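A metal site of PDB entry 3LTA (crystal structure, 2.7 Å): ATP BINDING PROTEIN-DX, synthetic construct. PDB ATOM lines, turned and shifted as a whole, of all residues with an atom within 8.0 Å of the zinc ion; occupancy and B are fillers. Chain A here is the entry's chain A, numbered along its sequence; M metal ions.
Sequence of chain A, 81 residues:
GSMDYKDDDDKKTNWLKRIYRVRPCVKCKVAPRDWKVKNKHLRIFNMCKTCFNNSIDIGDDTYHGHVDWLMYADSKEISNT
SG of Cys 25 lies close to N of Cys 48, 3.5 Å away.
The backbone carbonyl oxygen of Ala 31 is in hydrogen-bond range of the backbone NH of Cys 25 (2.7 Å).
The backbone NH of Lys 27 lies close to the side-chain sulfur of Cys 25.
N of Cys 51 lies within hydrogen-bond range of SG of Cys 48 (3.5 Å).
The side-chain sulfur of Cys 28 lies close to the backbone NH of Ala 31 (3.6 Å).
N of Val 30 lies close to SG of Cys 28 (3.7 Å).
The side-chain sulfur (SG) of Cys 48 sits close to the backbone NH (N) of Thr 50, 3.6 Å away.
Along chain A the residues within 4 Å of the zinc ion span positions 25 to 51.
The nearest printed residue that does not touch the zinc ion is Ala 31 (4.1 Å).
The zinc ion is bound by the side-chain sulfur (SG) of Cys 25 (2.2 Å), the side-chain sulfur (SG) of Cys 51 (2.3 Å) and the side-chain sulfur (SG) of Cys 28 (2.4 Å).
Slightly farther from the zinc ion lies the side-chain sulfur (SG) of Cys 48 (2.9 Å).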
ATOM      1  N   PRO A  24      25.737 -28.368 -22.787  1.00  0.00           N
ATOM      2  CA  PRO A  24      25.949 -27.532 -21.598  1.00  0.00           C
ATOM      3  C   PRO A  24      26.636 -26.208 -21.889  1.00  0.00           C
ATOM      4  O   PRO A  24      26.872 -25.850 -23.049  1.00  0.00           O
ATOM      5  CB  PRO A  24      26.913 -28.377 -20.744  1.00  0.00           C
ATOM      6  CG  PRO A  24      26.819 -29.745 -21.293  1.00  0.00           C
ATOM      7  CD  PRO A  24      26.559 -29.583 -22.764  1.00  0.00           C
ATOM      8  N   CYS A  25      26.951 -25.476 -20.823  1.00  0.00           N
ATOM      9  CA  CYS A  25      27.711 -24.264 -20.930  1.00  0.00           C
ATOM     10  C   CYS A  25      28.944 -24.442 -21.833  1.00  0.00           C
ATOM     11  O   CYS A  25      29.772 -25.303 -21.570  1.00  0.00           O
ATOM     12  CB  CYS A  25      28.190 -23.907 -19.536  1.00  0.00           C
ATOM     13  SG  CYS A  25      29.186 -22.413 -19.494  1.00  0.00           S
ATOM     14  N   VAL A  26      29.092 -23.611 -22.866  1.00  0.00           N
ATOM     15  CA  VAL A  26      30.300 -23.703 -23.698  1.00  0.00           C
ATOM     16  C   VAL A  26      31.622 -23.525 -22.925  1.00  0.00           C
ATOM     17  O   VAL A  26      32.688 -23.817 -23.457  1.00  0.00           O
ATOM     18  CB  VAL A  26      30.316 -22.640 -24.821  1.00  0.00           C
ATOM     19  CG1 VAL A  26      29.263 -22.941 -25.872  1.00  0.00           C
ATOM     20  CG2 VAL A  26      30.109 -21.284 -24.223  1.00  0.00           C
ATOM     21  N   LYS A  27      31.546 -23.030 -21.685  1.00  0.00           N
ATOM     22  CA  LYS A  27      32.750 -22.645 -20.943  1.00  0.00           C
ATOM     23  C   LYS A  27      33.127 -23.619 -19.847  1.00  0.00           C
ATOM     24  O   LYS A  27      34.250 -24.101 -19.825  1.00  0.00           O
ATOM     25  CB  LYS A  27      32.633 -21.237 -20.337  1.00  0.00           C
ATOM     26  CG  LYS A  27      33.831 -20.839 -19.442  1.00  0.00           C
ATOM     27  CD  LYS A  27      35.095 -20.615 -20.247  1.00  0.00           C
ATOM     28  CE  LYS A  27      36.327 -20.507 -19.373  1.00  0.00           C
ATOM     29  NZ  LYS A  27      37.542 -20.039 -20.121  1.00  0.00           N
ATOM     30  N   CYS A  28      32.232 -23.890 -18.911  1.00  0.00           N
ATOM     31  CA  CYS A  28      32.580 -24.815 -17.838  1.00  0.00           C
ATOM     32  C   CYS A  28      32.240 -26.225 -18.260  1.00  0.00           C
ATOM     33  O   CYS A  28      32.619 -27.191 -17.596  1.00  0.00           O
ATOM     34  CB  CYS A  28      31.859 -24.454 -16.527  1.00  0.00           C
ATOM     35  SG  CYS A  28      30.098 -24.903 -16.557  1.00  0.00           S
ATOM     36  N   LYS A  29      31.485 -26.339 -19.348  1.00  0.00           N
ATOM     37  CA  LYS A  29      31.154 -27.636 -19.941  1.00  0.00           C
ATOM     38  C   LYS A  29      30.306 -28.627 -19.140  1.00  0.00           C
ATOM     39  O   LYS A  29      30.050 -29.728 -19.630  1.00  0.00           O
ATOM     40  CB  LYS A  29      32.437 -28.334 -20.380  1.00  0.00           C
ATOM     41  CG  LYS A  29      33.239 -27.523 -21.375  1.00  0.00           C
ATOM     42  CD  LYS A  29      34.294 -28.343 -22.084  1.00  0.00           C
ATOM     43  CE  LYS A  29      35.031 -27.454 -23.045  1.00  0.00           C
ATOM     44  NZ  LYS A  29      34.047 -26.420 -23.483  1.00  0.00           N
ATOM     45  N   VAL A  30      29.883 -28.290 -17.920  1.00  0.00           N
ATOM     46  CA  VAL A  30      28.921 -29.171 -17.184  1.00  0.00           C
ATOM     47  C   VAL A  30      27.559 -28.519 -16.893  1.00  0.00           C
ATOM     48  O   VAL A  30      26.523 -29.016 -17.332  1.00  0.00           O
ATOM     49  CB  VAL A  30      29.536 -29.885 -15.933  1.00  0.00           C
ATOM     50  CG1 VAL A  30      30.526 -30.919 -16.385  1.00  0.00           C
ATOM     51  CG2 VAL A  30      30.208 -28.897 -14.993  1.00  0.00           C
ATOM     52  N   ALA A  31      27.553 -27.411 -16.143  1.00  0.00           N
ATOM     53  CA  ALA A  31      26.360 -26.580 -15.971  1.00  0.00           C
ATOM     54  C   ALA A  31      25.546 -26.404 -17.256  1.00  0.00           C
ATOM     55  O   ALA A  31      26.109 -26.272 -18.354  1.00  0.00           O
ATOM     56  CB  ALA A  31      26.757 -25.219 -15.402  1.00  0.00           C
ATOM     57  N   PRO A  32      24.209 -26.421 -17.134  1.00  0.00           N
ATOM     58  CA  PRO A  32      23.372 -26.169 -18.303  1.00  0.00           C
ATOM     59  C   PRO A  32      23.350 -24.674 -18.609  1.00  0.00           C
ATOM     60  O   PRO A  32      23.670 -23.862 -17.746  1.00  0.00           O
ATOM     61  CB  PRO A  32      21.994 -26.673 -17.855  1.00  0.00           C
ATOM     62  CG  PRO A  32      21.996 -26.526 -16.361  1.00  0.00           C
ATOM     63  CD  PRO A  32      23.430 -26.733 -15.922  1.00  0.00           C
ATOM     64  N   ARG A  33      22.994 -24.289 -19.825  1.00  0.00           N
ATOM     65  CA  ARG A  33      23.028 -22.876 -20.205  1.00  0.00           C
ATOM     66  C   ARG A  33      21.926 -22.020 -19.577  1.00  0.00           C
ATOM     67  O   ARG A  33      20.842 -22.492 -19.214  1.00  0.00           O
ATOM     68  CB  ARG A  33      22.972 -22.729 -21.709  1.00  0.00           C
ATOM     69  CG  ARG A  33      24.096 -23.449 -22.401  1.00  0.00           C
ATOM     70  CD  ARG A  33      24.032 -23.349 -23.890  1.00  0.00           C
ATOM     71  NE  ARG A  33      25.110 -24.159 -24.426  1.00  0.00           N
ATOM     72  CZ  ARG A  33      25.512 -24.169 -25.690  1.00  0.00           C
ATOM     73  NH1 ARG A  33      24.930 -23.386 -26.597  1.00  0.00           N
ATOM     74  NH2 ARG A  33      26.521 -24.952 -26.019  1.00  0.00           N
ATOM     75  N   ASP A  34      22.224 -20.733 -19.459  1.00  0.00           N
ATOM     76  CA  ASP A  34      21.209 -19.781 -19.096  1.00  0.00           C
ATOM     77  C   ASP A  34      20.328 -19.552 -20.307  1.00  0.00           C
ATOM     78  O   ASP A  34      20.763 -19.708 -21.436  1.00  0.00           O
ATOM     79  CB  ASP A  34      21.867 -18.469 -18.680  1.00  0.00           C
ATOM     80  CG  ASP A  34      21.006 -17.679 -17.727  1.00  0.00           C
ATOM     81  OD1 ASP A  34      19.785 -17.918 -17.621  1.00  0.00           O
ATOM     82  OD2 ASP A  34      21.566 -16.777 -17.066  1.00  0.00           O
ATOM     83  N   ASN A  46      24.935 -18.852 -24.397  1.00  0.00           N
ATOM     84  CA  ASN A  46      26.045 -19.775 -24.526  1.00  0.00           C
ATOM     85  C   ASN A  46      26.549 -20.389 -23.201  1.00  0.00           C
ATOM     86  O   ASN A  46      26.981 -21.566 -23.158  1.00  0.00           O
ATOM     87  CB  ASN A  46      27.187 -19.096 -25.299  1.00  0.00           C
ATOM     88  CG  ASN A  46      26.822 -18.843 -26.737  1.00  0.00           C
ATOM     89  OD1 ASN A  46      25.865 -19.422 -27.252  1.00  0.00           O
ATOM     90  ND2 ASN A  46      27.565 -17.965 -27.391  1.00  0.00           N
ATOM     91  N   MET A  47      26.482 -19.596 -22.134  1.00  0.00           N
ATOM     92  CA  MET A  47      27.050 -19.939 -20.843  1.00  0.00           C
ATOM     93  C   MET A  47      26.012 -19.951 -19.732  1.00  0.00           C
ATOM     94  O   MET A  47      25.011 -19.254 -19.807  1.00  0.00           O
ATOM     95  CB  MET A  47      28.107 -18.915 -20.488  1.00  0.00           C
ATOM     96  CG  MET A  47      29.519 -19.364 -20.771  1.00  0.00           C
ATOM     97  SD  MET A  47      30.696 -18.043 -21.110  1.00  0.00           S
ATOM     98  CE  MET A  47      30.004 -16.638 -20.248  1.00  0.00           C
ATOM     99  N   CYS A  48      26.265 -20.736 -18.682  1.00  0.00           N
ATOM    100  CA  CYS A  48      25.414 -20.647 -17.479  1.00  0.00           C
ATOM    101  C   CYS A  48      25.606 -19.250 -16.884  1.00  0.00           C
ATOM    102  O   CYS A  48      26.402 -18.456 -17.382  1.00  0.00           O
ATOM    103  CB  CYS A  48      25.762 -21.738 -16.461  1.00  0.00           C
ATOM    104  SG  CYS A  48      27.329 -21.468 -15.662  1.00  0.00           S
ATOM    105  N   LYS A  49      24.883 -18.908 -15.829  1.00  0.00           N
ATOM    106  CA  LYS A  49      25.015 -17.542 -15.367  1.00  0.00           C
ATOM    107  C   LYS A  49      26.344 -17.298 -14.624  1.00  0.00           C
ATOM    108  O   LYS A  49      26.939 -16.206 -14.713  1.00  0.00           O
ATOM    109  CB  LYS A  49      23.845 -17.119 -14.510  1.00  0.00           C
ATOM    110  CG  LYS A  49      24.057 -15.734 -13.955  1.00  0.00           C
ATOM    111  CD  LYS A  49      23.032 -15.431 -12.916  1.00  0.00           C
ATOM    112  CE  LYS A  49      22.996 -13.949 -12.600  1.00  0.00           C
ATOM    113  NZ  LYS A  49      22.015 -13.737 -11.508  1.00  0.00           N
ATOM    114  N   THR A  50      26.817 -18.318 -13.909  1.00  0.00           N
ATOM    115  CA  THR A  50      28.039 -18.149 -13.146  1.00  0.00           C
ATOM    116  C   THR A  50      29.251 -17.883 -14.044  1.00  0.00           C
ATOM    117  O   THR A  50      29.992 -16.903 -13.829  1.00  0.00           O
ATOM    118  CB  THR A  50      28.304 -19.347 -12.278  1.00  0.00           C
ATOM    119  OG1 THR A  50      27.221 -19.463 -11.342  1.00  0.00           O
ATOM    120  CG2 THR A  50      29.587 -19.150 -11.487  1.00  0.00           C
ATOM    121  N   CYS A  51      29.436 -18.749 -15.046  1.00  0.00           N
ATOM    122  CA  CYS A  51      30.511 -18.544 -16.030  1.00  0.00           C
ATOM    123  C   CYS A  51      30.297 -17.228 -16.770  1.00  0.00           C
ATOM    124  O   CYS A  51      31.264 -16.539 -17.083  1.00  0.00           O
ATOM    125  CB  CYS A  51      30.624 -19.700 -17.014  1.00  0.00           C
ATOM    126  SG  CYS A  51      30.972 -21.342 -16.282  1.00  0.00           S
ATOM    127  N   PHE A  52      29.046 -16.859 -17.052  1.00  0.00           N
ATOM    128  CA  PHE A  52      28.874 -15.570 -17.713  1.00  0.00           C
ATOM    129  C   PHE A  52      29.423 -14.370 -16.911  1.00  0.00           C
ATOM    130  O   PHE A  52      30.255 -13.604 -17.413  1.00  0.00           O
ATOM    131  CB  PHE A  52      27.437 -15.300 -18.129  1.00  0.00           C
ATOM    132  CG  PHE A  52      27.266 -13.962 -18.827  1.00  0.00           C
ATOM    133  CD1 PHE A  52      27.916 -13.706 -20.032  1.00  0.00           C
ATOM    134  CD2 PHE A  52      26.483 -12.949 -18.259  1.00  0.00           C
ATOM    135  CE1 PHE A  52      27.771 -12.471 -20.690  1.00  0.00           C
ATOM    136  CE2 PHE A  52      26.325 -11.707 -18.908  1.00  0.00           C
ATOM    137  CZ  PHE A  52      26.983 -11.472 -20.119  1.00  0.00           C
HETATM  138 ZN    ZN M   1      29.360 -22.716 -17.294  1.00  0.00          ZN
